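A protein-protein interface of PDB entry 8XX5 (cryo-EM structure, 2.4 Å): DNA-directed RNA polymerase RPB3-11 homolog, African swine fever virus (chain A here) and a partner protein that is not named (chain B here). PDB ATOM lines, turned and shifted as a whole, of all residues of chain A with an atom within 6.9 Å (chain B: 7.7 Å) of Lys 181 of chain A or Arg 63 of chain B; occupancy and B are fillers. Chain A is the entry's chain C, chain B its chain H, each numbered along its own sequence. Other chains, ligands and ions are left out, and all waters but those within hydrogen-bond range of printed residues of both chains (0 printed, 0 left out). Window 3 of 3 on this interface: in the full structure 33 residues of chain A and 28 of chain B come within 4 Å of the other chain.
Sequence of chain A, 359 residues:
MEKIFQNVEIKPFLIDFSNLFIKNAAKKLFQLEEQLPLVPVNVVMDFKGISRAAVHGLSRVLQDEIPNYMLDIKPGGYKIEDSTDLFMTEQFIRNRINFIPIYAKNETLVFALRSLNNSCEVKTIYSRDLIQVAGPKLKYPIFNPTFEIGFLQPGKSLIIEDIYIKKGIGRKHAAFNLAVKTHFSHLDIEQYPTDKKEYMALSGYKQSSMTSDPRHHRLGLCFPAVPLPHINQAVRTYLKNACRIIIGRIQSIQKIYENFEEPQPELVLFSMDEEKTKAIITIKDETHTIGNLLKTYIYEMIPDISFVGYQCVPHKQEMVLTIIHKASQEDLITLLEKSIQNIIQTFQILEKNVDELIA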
ATOM      1  N   PHE A  13     -14.744  23.194 -26.423  1.00  0.00           N
ATOM      2  CA  PHE A  13     -14.646  22.316 -27.580  1.00  0.00           C
ATOM      3  C   PHE A  13     -14.130  23.132 -28.758  1.00  0.00           C
ATOM      4  O   PHE A  13     -14.775  24.099 -29.177  1.00  0.00           O
ATOM      5  CB  PHE A  13     -16.001  21.689 -27.906  1.00  0.00           C
ATOM      6  CG  PHE A  13     -16.451  20.672 -26.902  1.00  0.00           C
ATOM      7  CD1 PHE A  13     -15.555  19.763 -26.372  1.00  0.00           C
ATOM      8  CD2 PHE A  13     -17.766  20.633 -26.479  1.00  0.00           C
ATOM      9  CE1 PHE A  13     -15.965  18.829 -25.445  1.00  0.00           C
ATOM     10  CE2 PHE A  13     -18.180  19.700 -25.552  1.00  0.00           C
ATOM     11  CZ  PHE A  13     -17.281  18.797 -25.035  1.00  0.00           C
ATOM     12  N   ASN A  42     -17.398  22.611 -22.037  1.00  0.00           N
ATOM     13  CA  ASN A  42     -17.754  21.506 -21.159  1.00  0.00           C
ATOM     14  C   ASN A  42     -17.347  21.868 -19.738  1.00  0.00           C
ATOM     15  O   ASN A  42     -16.170  22.127 -19.472  1.00  0.00           O
ATOM     16  CB  ASN A  42     -17.079  20.212 -21.604  1.00  0.00           C
ATOM     17  CG  ASN A  42     -17.621  19.000 -20.883  1.00  0.00           C
ATOM     18  OD1 ASN A  42     -18.827  18.875 -20.687  1.00  0.00           O
ATOM     19  ND2 ASN A  42     -16.733  18.101 -20.480  1.00  0.00           N
ATOM     20  N   HIS A  56     -29.089  17.538  -8.862  1.00  0.00           N
ATOM     21  CA  HIS A  56     -29.882  17.234 -10.046  1.00  0.00           C
ATOM     22  C   HIS A  56     -30.868  18.348 -10.367  1.00  0.00           C
ATOM     23  O   HIS A  56     -31.166  18.578 -11.539  1.00  0.00           O
ATOM     24  CB  HIS A  56     -30.624  15.912  -9.887  1.00  0.00           C
ATOM     25  CG  HIS A  56     -31.366  15.503 -11.120  1.00  0.00           C
ATOM     26  ND1 HIS A  56     -30.752  15.381 -12.347  1.00  0.00           N
ATOM     27  CD2 HIS A  56     -32.673  15.219 -11.323  1.00  0.00           C
ATOM     28  CE1 HIS A  56     -31.646  15.025 -13.251  1.00  0.00           C
ATOM     29  NE2 HIS A  56     -32.819  14.918 -12.656  1.00  0.00           N
ATOM     30  N   SER A  59     -28.903  20.823 -12.219  1.00  0.00           N
ATOM     31  CA  SER A  59     -28.706  20.325 -13.576  1.00  0.00           C
ATOM     32  C   SER A  59     -29.955  20.519 -14.429  1.00  0.00           C
ATOM     33  O   SER A  59     -29.867  20.960 -15.579  1.00  0.00           O
ATOM     34  CB  SER A  59     -28.305  18.851 -13.533  1.00  0.00           C
ATOM     35  OG  SER A  59     -28.459  18.240 -14.800  1.00  0.00           O
ATOM     36  N   GLN A  63     -30.445  22.876 -17.658  1.00  0.00           N
ATOM     37  CA  GLN A  63     -30.866  22.250 -18.902  1.00  0.00           C
ATOM     38  C   GLN A  63     -32.024  23.002 -19.539  1.00  0.00           C
ATOM     39  O   GLN A  63     -31.884  23.549 -20.636  1.00  0.00           O
ATOM     40  CB  GLN A  63     -31.279  20.798 -18.664  1.00  0.00           C
ATOM     41  CG  GLN A  63     -30.134  19.821 -18.525  1.00  0.00           C
ATOM     42  CD  GLN A  63     -30.592  18.495 -17.963  1.00  0.00           C
ATOM     43  OE1 GLN A  63     -31.392  17.793 -18.578  1.00  0.00           O
ATOM     44  NE2 GLN A  63     -30.097  18.150 -16.784  1.00  0.00           N
ATOM     45  N   ALA A 179     -28.124  23.925 -21.338  1.00  0.00           N
ATOM     46  CA  ALA A 179     -27.039  22.993 -21.072  1.00  0.00           C
ATOM     47  C   ALA A 179     -27.453  21.584 -21.468  1.00  0.00           C
ATOM     48  O   ALA A 179     -28.565  21.149 -21.156  1.00  0.00           O
ATOM     49  CB  ALA A 179     -26.635  23.030 -19.598  1.00  0.00           C
ATOM     50  N   VAL A 180     -26.561  20.881 -22.157  1.00  0.00           N
ATOM     51  CA  VAL A 180     -26.762  19.479 -22.499  1.00  0.00           C
ATOM     52  C   VAL A 180     -25.953  18.636 -21.524  1.00  0.00           C
ATOM     53  O   VAL A 180     -24.844  19.014 -21.126  1.00  0.00           O
ATOM     54  CB  VAL A 180     -26.381  19.194 -23.969  1.00  0.00           C
ATOM     55  CG1 VAL A 180     -26.176  20.494 -24.732  1.00  0.00           C
ATOM     56  CG2 VAL A 180     -25.155  18.298 -24.077  1.00  0.00           C
ATOM     57  N   LYS A 181     -26.529  17.514 -21.101  1.00  0.00           N
ATOM     58  CA  LYS A 181     -25.896  16.685 -20.085  1.00  0.00           C
ATOM     59  C   LYS A 181     -24.670  15.984 -20.653  1.00  0.00           C
ATOM     60  O   LYS A 181     -24.722  15.391 -21.734  1.00  0.00           O
ATOM     61  CB  LYS A 181     -26.889  15.658 -19.545  1.00  0.00           C
ATOM     62  CG  LYS A 181     -28.049  16.268 -18.786  1.00  0.00           C
ATOM     63  CD  LYS A 181     -29.080  15.223 -18.412  1.00  0.00           C
ATOM     64  CE  LYS A 181     -29.998  14.910 -19.579  1.00  0.00           C
ATOM     65  NZ  LYS A 181     -30.431  16.134 -20.297  1.00  0.00           N
ATOM     66  N   THR A 182     -23.571  16.050 -19.917  1.00  0.00           N
ATOM     67  CA  THR A 182     -22.317  15.426 -20.313  1.00  0.00           C
ATOM     68  C   THR A 182     -21.867  14.341 -19.351  1.00  0.00           C
ATOM     69  O   THR A 182     -21.408  13.285 -19.791  1.00  0.00           O
ATOM     70  CB  THR A 182     -21.218  16.496 -20.441  1.00  0.00           C
ATOM     71  OG1 THR A 182     -21.238  17.045 -21.765  1.00  0.00           O
ATOM     72  CG2 THR A 182     -19.843  15.912 -20.161  1.00  0.00           C
ATOM     73  N   HIS A 183     -22.003  14.563 -18.048  1.00  0.00           N
ATOM     74  CA  HIS A 183     -21.556  13.590 -17.066  1.00  0.00           C
ATOM     75  C   HIS A 183     -22.381  13.736 -15.799  1.00  0.00           C
ATOM     76  O   HIS A 183     -22.777  14.844 -15.429  1.00  0.00           O
ATOM     77  CB  HIS A 183     -20.067  13.764 -16.750  1.00  0.00           C
ATOM     78  CG  HIS A 183     -19.534  12.751 -15.790  1.00  0.00           C
ATOM     79  ND1 HIS A 183     -19.256  11.452 -16.156  1.00  0.00           N
ATOM     80  CD2 HIS A 183     -19.235  12.841 -14.473  1.00  0.00           C
ATOM     81  CE1 HIS A 183     -18.805  10.787 -15.109  1.00  0.00           C
ATOM     82  NE2 HIS A 183     -18.783  11.608 -14.074  1.00  0.00           N
ATOM     83  N   PHE A 184     -22.640  12.609 -15.145  1.00  0.00           N
ATOM     84  CA  PHE A 184     -23.255  12.599 -13.826  1.00  0.00           C
ATOM     85  C   PHE A 184     -22.813  11.335 -13.112  1.00  0.00           C
ATOM     86  O   PHE A 184     -23.001  10.231 -13.628  1.00  0.00           O
ATOM     87  CB  PHE A 184     -24.782  12.660 -13.909  1.00  0.00           C
ATOM     88  CG  PHE A 184     -25.447  12.860 -12.579  1.00  0.00           C
ATOM     89  CD1 PHE A 184     -25.045  13.882 -11.738  1.00  0.00           C
ATOM     90  CD2 PHE A 184     -26.467  12.023 -12.167  1.00  0.00           C
ATOM     91  CE1 PHE A 184     -25.650  14.067 -10.513  1.00  0.00           C
ATOM     92  CE2 PHE A 184     -27.078  12.204 -10.942  1.00  0.00           C
ATOM     93  CZ  PHE A 184     -26.669  13.228 -10.114  1.00  0.00           C
ATOM     94  N   LEU A 219     -20.891  16.590 -11.709  1.00  0.00           N
ATOM     95  CA  LEU A 219     -21.870  16.976 -12.714  1.00  0.00           C
ATOM     96  C   LEU A 219     -21.155  17.572 -13.915  1.00  0.00           C
ATOM     97  O   LEU A 219     -20.377  18.521 -13.772  1.00  0.00           O
ATOM     98  CB  LEU A 219     -22.880  17.974 -12.144  1.00  0.00           C
ATOM     99  CG  LEU A 219     -23.872  18.585 -13.135  1.00  0.00           C
ATOM    100  CD1 LEU A 219     -24.669  17.498 -13.831  1.00  0.00           C
ATOM    101  CD2 LEU A 219     -24.797  19.555 -12.424  1.00  0.00           C
ATOM    102  N   GLY A 220     -21.416  17.013 -15.091  1.00  0.00           N
ATOM    103  CA  GLY A 220     -20.862  17.537 -16.321  1.00  0.00           C
ATOM    104  C   GLY A 220     -21.928  18.100 -17.236  1.00  0.00           C
ATOM    105  O   GLY A 220     -22.849  17.384 -17.639  1.00  0.00           O
ATOM    106  N   LEU A 221     -21.822  19.382 -17.564  1.00  0.00           N
ATOM    107  CA  LEU A 221     -22.774  20.050 -18.437  1.00  0.00           C
ATOM    108  C   LEU A 221     -22.021  20.815 -19.511  1.00  0.00           C
ATOM    109  O   LEU A 221     -20.991  21.437 -19.236  1.00  0.00           O
ATOM    110  CB  LEU A 221     -23.679  21.002 -17.650  1.00  0.00           C
ATOM    111  CG  LEU A 221     -24.744  20.348 -16.770  1.00  0.00           C
ATOM    112  CD1 LEU A 221     -25.444  21.386 -15.919  1.00  0.00           C
ATOM    113  CD2 LEU A 221     -25.749  19.585 -17.615  1.00  0.00           C
ATOM    114  N   CYS A 222     -22.535  20.765 -20.735  1.00  0.00           N
ATOM    115  CA  CYS A 222     -21.944  21.468 -21.864  1.00  0.00           C
ATOM    116  C   CYS A 222     -22.837  22.630 -22.268  1.00  0.00           C
ATOM    117  O   CYS A 222     -24.048  22.459 -22.442  1.00  0.00           O
ATOM    118  CB  CYS A 222     -21.736  20.527 -23.051  1.00  0.00           C
ATOM    119  SG  CYS A 222     -21.043  21.335 -24.506  1.00  0.00           S
ATOM    120  N   CYS B   7     -28.186  18.808 -32.533  1.00  0.00           N
ATOM    121  CA  CYS B   7     -28.508  17.395 -32.409  1.00  0.00           C
ATOM    122  C   CYS B   7     -29.949  17.229 -31.945  1.00  0.00           C
ATOM    123  O   CYS B   7     -30.387  17.885 -30.997  1.00  0.00           O
ATOM    124  CB  CYS B   7     -27.550  16.726 -31.427  1.00  0.00           C
ATOM    125  SG  CYS B   7     -28.004  15.046 -30.964  1.00  0.00           S
ATOM    126  N   THR B   9     -31.341  14.899 -30.369  1.00  0.00           N
ATOM    127  CA  THR B   9     -31.506  14.200 -29.104  1.00  0.00           C
ATOM    128  C   THR B   9     -31.125  15.056 -27.902  1.00  0.00           C
ATOM    129  O   THR B   9     -31.835  15.058 -26.892  1.00  0.00           O
ATOM    130  CB  THR B   9     -30.679  12.914 -29.115  1.00  0.00           C
ATOM    131  OG1 THR B   9     -30.830  12.260 -30.380  1.00  0.00           O
ATOM    132  CG2 THR B   9     -31.145  11.991 -28.027  1.00  0.00           C
ATOM    133  N   CYS B  10     -30.013  15.782 -27.987  1.00  0.00           N
ATOM    134  CA  CYS B  10     -29.520  16.546 -26.853  1.00  0.00           C
ATOM    135  C   CYS B  10     -29.386  18.038 -27.120  1.00  0.00           C
ATOM    136  O   CYS B  10     -29.178  18.796 -26.168  1.00  0.00           O
ATOM    137  CB  CYS B  10     -28.160  16.001 -26.394  1.00  0.00           C
ATOM    138  SG  CYS B  10     -26.818  16.319 -27.541  1.00  0.00           S
ATOM    139  N   GLY B  11     -29.504  18.481 -28.368  1.00  0.00           N
ATOM    140  CA  GLY B  11     -29.424  19.893 -28.670  1.00  0.00           C
ATOM    141  C   GLY B  11     -28.028  20.449 -28.817  1.00  0.00           C
ATOM    142  O   GLY B  11     -27.869  21.674 -28.827  1.00  0.00           O
ATOM    143  N   PHE B  12     -27.013  19.599 -28.918  1.00  0.00           N
ATOM    144  CA  PHE B  12     -25.666  20.086 -29.164  1.00  0.00           C
ATOM    145  C   PHE B  12     -25.583  20.688 -30.566  1.00  0.00           C
ATOM    146  O   PHE B  12     -26.097  20.105 -31.523  1.00  0.00           O
ATOM    147  CB  PHE B  12     -24.648  18.958 -29.014  1.00  0.00           C
ATOM    148  CG  PHE B  12     -23.221  19.412 -29.121  1.00  0.00           C
ATOM    149  CD1 PHE B  12     -22.527  19.824 -27.998  1.00  0.00           C
ATOM    150  CD2 PHE B  12     -22.574  19.430 -30.345  1.00  0.00           C
ATOM    151  CE1 PHE B  12     -21.219  20.245 -28.093  1.00  0.00           C
ATOM    152  CE2 PHE B  12     -21.267  19.851 -30.445  1.00  0.00           C
ATOM    153  CZ  PHE B  12     -20.587  20.259 -29.317  1.00  0.00           C
ATOM    154  N   ILE B  14     -24.504  20.657 -33.574  1.00  0.00           N
ATOM    155  CA  ILE B  14     -23.750  19.948 -34.600  1.00  0.00           C
ATOM    156  C   ILE B  14     -23.761  20.696 -35.925  1.00  0.00           C
ATOM    157  O   ILE B  14     -22.904  20.446 -36.779  1.00  0.00           O
ATOM    158  CB  ILE B  14     -24.292  18.519 -34.782  1.00  0.00           C
ATOM    159  CG1 ILE B  14     -25.794  18.545 -35.064  1.00  0.00           C
ATOM    160  CG2 ILE B  14     -23.990  17.678 -33.555  1.00  0.00           C
ATOM    161  CD1 ILE B  14     -26.293  17.334 -35.811  1.00  0.00           C
ATOM    162  N   ILE B  55     -14.690  13.660 -37.136  1.00  0.00           N
ATOM    163  CA  ILE B  55     -15.632  14.266 -36.199  1.00  0.00           C
ATOM    164  C   ILE B  55     -14.907  14.749 -34.952  1.00  0.00           C
ATOM    165  O   ILE B  55     -15.192  15.836 -34.433  1.00  0.00           O
ATOM    166  CB  ILE B  55     -16.757  13.274 -35.854  1.00  0.00           C
ATOM    167  CG1 ILE B  55     -17.473  12.815 -37.123  1.00  0.00           C
ATOM    168  CG2 ILE B  55     -17.751  13.907 -34.904  1.00  0.00           C
ATOM    169  CD1 ILE B  55     -18.148  11.477 -36.980  1.00  0.00           C
ATOM    170  N   ILE B  60     -16.530  18.008 -32.145  1.00  0.00           N
ATOM    171  CA  ILE B  60     -17.759  17.364 -31.671  1.00  0.00           C
ATOM    172  C   ILE B  60     -17.392  16.271 -30.672  1.00  0.00           C
ATOM    173  O   ILE B  60     -16.463  15.487 -30.930  1.00  0.00           O
ATOM    174  CB  ILE B  60     -18.547  16.796 -32.854  1.00  0.00           C
ATOM    175  CG1 ILE B  60     -19.165  17.934 -33.666  1.00  0.00           C
ATOM    176  CG2 ILE B  60     -19.626  15.836 -32.386  1.00  0.00           C
ATOM    177  CD1 ILE B  60     -19.003  17.775 -35.156  1.00  0.00           C
ATOM    178  N   PRO B  61     -18.068  16.182 -29.529  1.00  0.00           N
ATOM    179  CA  PRO B  61     -17.695  15.182 -28.523  1.00  0.00           C
ATOM    180  C   PRO B  61     -18.056  13.776 -28.974  1.00  0.00           C
ATOM    181  O   PRO B  61     -18.789  13.563 -29.942  1.00  0.00           O
ATOM    182  CB  PRO B  61     -18.505  15.591 -27.288  1.00  0.00           C
ATOM    183  CG  PRO B  61     -19.047  16.959 -27.592  1.00  0.00           C
ATOM    184  CD  PRO B  61     -19.177  17.031 -29.071  1.00  0.00           C
ATOM    185  N   MET B  62     -17.521  12.799 -28.244  1.00  0.00           N
ATOM    186  CA  MET B  62     -17.861  11.401 -28.476  1.00  0.00           C
ATOM    187  C   MET B  62     -19.260  11.081 -27.969  1.00  0.00           C
ATOM    188  O   MET B  62     -19.421  10.333 -26.999  1.00  0.00           O
ATOM    189  CB  MET B  62     -16.843  10.479 -27.808  1.00  0.00           C
ATOM    190  CG  MET B  62     -15.718  10.029 -28.714  1.00  0.00           C
ATOM    191  SD  MET B  62     -16.342   8.982 -30.042  1.00  0.00           S
ATOM    192  CE  MET B  62     -15.718   7.388 -29.521  1.00  0.00           C
ATOM    193  N   ARG B  63     -20.274  11.638 -28.618  1.00  0.00           N
ATOM    194  CA  ARG B  63     -21.664  11.408 -28.259  1.00  0.00           C
ATOM    195  C   ARG B  63     -22.331  10.608 -29.367  1.00  0.00           C
ATOM    196  O   ARG B  63     -22.208  10.955 -30.544  1.00  0.00           O
ATOM    197  CB  ARG B  63     -22.395  12.732 -28.034  1.00  0.00           C
ATOM    198  CG  ARG B  63     -21.822  13.554 -26.895  1.00  0.00           C
ATOM    199  CD  ARG B  63     -22.419  14.948 -26.851  1.00  0.00           C
ATOM    200  NE  ARG B  63     -23.807  14.925 -26.409  1.00  0.00           N
ATOM    201  CZ  ARG B  63     -24.194  14.725 -25.156  1.00  0.00           C
ATOM    202  NH1 ARG B  63     -23.318  14.537 -24.183  1.00  0.00           N
ATOM    203  NH2 ARG B  63     -25.491  14.710 -24.873  1.00  0.00           N
ATOM    204  N   VAL B  64     -23.032   9.540 -28.985  1.00  0.00           N
ATOM    205  CA  VAL B  64     -23.668   8.671 -29.972  1.00  0.00           C
ATOM    206  C   VAL B  64     -24.656   9.467 -30.816  1.00  0.00           C
ATOM    207  O   VAL B  64     -24.651   9.392 -32.052  1.00  0.00           O
ATOM    208  CB  VAL B  64     -24.352   7.483 -29.273  1.00  0.00           C
ATOM    209  CG1 VAL B  64     -25.245   6.731 -30.240  1.00  0.00           C
ATOM    210  CG2 VAL B  64     -23.314   6.556 -28.669  1.00  0.00           C
ATOM    211  N   CYS B  65     -25.493  10.268 -30.156  1.00  0.00           N
ATOM    212  CA  CYS B  65     -26.534  11.016 -30.852  1.00  0.00           C
ATOM    213  C   CYS B  65     -25.944  12.019 -31.834  1.00  0.00           C
ATOM    214  O   CYS B  65     -26.383  12.110 -32.988  1.00  0.00           O
ATOM    215  CB  CYS B  65     -27.414  11.728 -29.827  1.00  0.00           C
ATOM    216  SG  CYS B  65     -26.483  12.646 -28.569  1.00  0.00           S
ATOM    217  N   CYS B  66     -24.949  12.786 -31.391  1.00  0.00           N
ATOM    218  CA  CYS B  66     -24.426  13.874 -32.211  1.00  0.00           C
ATOM    219  C   CYS B  66     -23.717  13.340 -33.447  1.00  0.00           C
ATOM    220  O   CYS B  66     -23.963  13.807 -34.565  1.00  0.00           O
ATOM    221  CB  CYS B  66     -23.482  14.742 -31.381  1.00  0.00           C
ATOM    222  SG  CYS B  66     -24.286  15.556 -29.999  1.00  0.00           S
ATOM    223  N   ARG B  67     -22.836  12.356 -33.265  1.00  0.00           N
ATOM    224  CA  ARG B  67     -22.143  11.769 -34.405  1.00  0.00           C
ATOM    225  C   ARG B  67     -23.115  11.054 -35.332  1.00  0.00           C
ATOM    226  O   ARG B  67     -22.968  11.118 -36.559  1.00  0.00           O
ATOM    227  CB  ARG B  67     -21.052  10.821 -33.917  1.00  0.00           C
ATOM    228  CG  ARG B  67     -20.169  11.429 -32.850  1.00  0.00           C
ATOM    229  CD  ARG B  67     -18.756  10.911 -32.929  1.00  0.00           C
ATOM    230  NE  ARG B  67     -17.844  11.750 -32.165  1.00  0.00           N
ATOM    231  CZ  ARG B  67     -16.531  11.776 -32.336  1.00  0.00           C
ATOM    232  NH1 ARG B  67     -15.939  11.013 -33.239  1.00  0.00           N
ATOM    233  NH2 ARG B  67     -15.795  12.587 -31.584  1.00  0.00           N
ATOM    234  N   THR B  68     -24.113  10.370 -34.768  1.00  0.00           N
ATOM    235  CA  THR B  68     -25.127   9.726 -35.595  1.00  0.00           C
ATOM    236  C   THR B  68     -25.826  10.737 -36.493  1.00  0.00           C
ATOM    237  O   THR B  68     -25.902  10.557 -37.716  1.00  0.00           O
ATOM    238  CB  THR B  68     -26.145   9.012 -34.710  1.00  0.00           C
ATOM    239  OG1 THR B  68     -25.511   7.935 -34.015  1.00  0.00           O
ATOM    240  CG2 THR B  68     -27.272   8.469 -35.548  1.00  0.00           C
ATOM    241  N   HIS B  69     -26.335  11.820 -35.901  1.00  0.00           N
ATOM    242  CA  HIS B  69     -27.072  12.808 -36.679  1.00  0.00           C
ATOM    243  C   HIS B  69     -26.164  13.559 -37.640  1.00  0.00           C
ATOM    244  O   HIS B  69     -26.627  14.036 -38.682  1.00  0.00           O
ATOM    245  CB  HIS B  69     -27.790  13.781 -35.745  1.00  0.00           C
ATOM    246  CG  HIS B  69     -28.848  13.136 -34.907  1.00  0.00           C
ATOM    247  ND1 HIS B  69     -29.583  12.053 -35.341  1.00  0.00           N
ATOM    248  CD2 HIS B  69     -29.291  13.413 -33.658  1.00  0.00           C
ATOM    249  CE1 HIS B  69     -30.435  11.695 -34.398  1.00  0.00           C
ATOM    250  NE2 HIS B  69     -30.277  12.503 -33.366  1.00  0.00           N
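Of the printed residues of chain B, Phe 13 of chain A touches Phe 12 (3.8 Å) and Pro 61 (3.5 Å).
Of the printed residues of chain B, Val 180 of chain A touches Cys 10 and Arg 63.
Of chain B, only Arg 63 comes within 4 Å of Lys 181 of chain A.
Printed residues of chain B within 4 Å of Cys 222 of chain A: Phe 12.
Thr 9 of chain B touches none of the printed residues of chain A.
Printed residues of chain A within 4 Å of Phe 12 of chain B: Phe 13 and Cys 222.
Printed residues of chain A within 4 Å of Pro 61 of chain B: Phe 13 (3.5 Å).
Arg 63 of chain B touches just these residues of chain A: Val 180 (3.7 Å) and Lys 181 (2.9 Å).
Cys 66 of chain B touches none of the printed residues of chain A.
The nearest residue of chain B that does not touch Lys 181 of chain A is Cys 10 of chain B (5.7 Å).
The nearest residue of chain A that does not touch Arg 63 of chain B is Thr 182 of chain A (4.1 Å).
The backbone carbonyl oxygen of Lys 181 of chain A lies within hydrogen-bond range of the guanidinium group of Arg 63 of chain B, at 2.9 Å.
Among the printed residues, merely in contact across the chains: Phe 13 of chain A with Phe 12 of chain B (3.8 Å), Phe 13 of chain A with Pro 61 of chain B (3.5 Å), Val 180 of chain A with Cys 10 of chain B (3.6 Å), Val 180 of chain A with Arg 63 of chain B (3.7 Å) and Cys 222 of chain A with Phe 12 of chain B (3.8 Å).
Of the 17 printed residues of chain B, 4 touch a printed residue of chain A.
Hydrophobic or aromatic side chains of chain B that line the printed part of chain A: Phe 12 and Pro 61.
Hydrophobic or aromatic side chains of chain A within 4 Å of the printed part of chain B: Phe 13 and Val 180.
Along chain A the printed residues that touch a printed residue of chain B span positions 13 to 222.
Among the printed residues, no Asp or Glu carboxylate lies within 4 Å of a Lys or Arg side-chain nitrogen of the other chain.
O of Pro 61 of chain B lies within hydrogen-bond range of NE of Arg 67 of chain B (3.0 Å).
SG of Cys 10 of chain B sits close to N of Phe 12 of chain B (3.6 Å).
The side-chain amide oxygen of Gln 63 of chain A is in hydrogen-bond range of the side-chain amino group of Lys 181 of chain A (2.6 Å).
NE of Arg 63 of chain B sits close to SG of Cys 66 of chain B.
The guanidinium group of Arg 63 of chain B lies close to the side-chain sulfur of Cys 10 of chain B, at 3.4 Å.
The backbone NH (N) of Cys 7 of chain B sits at hydrogen-bond distance from the backbone carbonyl oxygen (O) of Phe 12 of chain B, 2.7 Å away.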
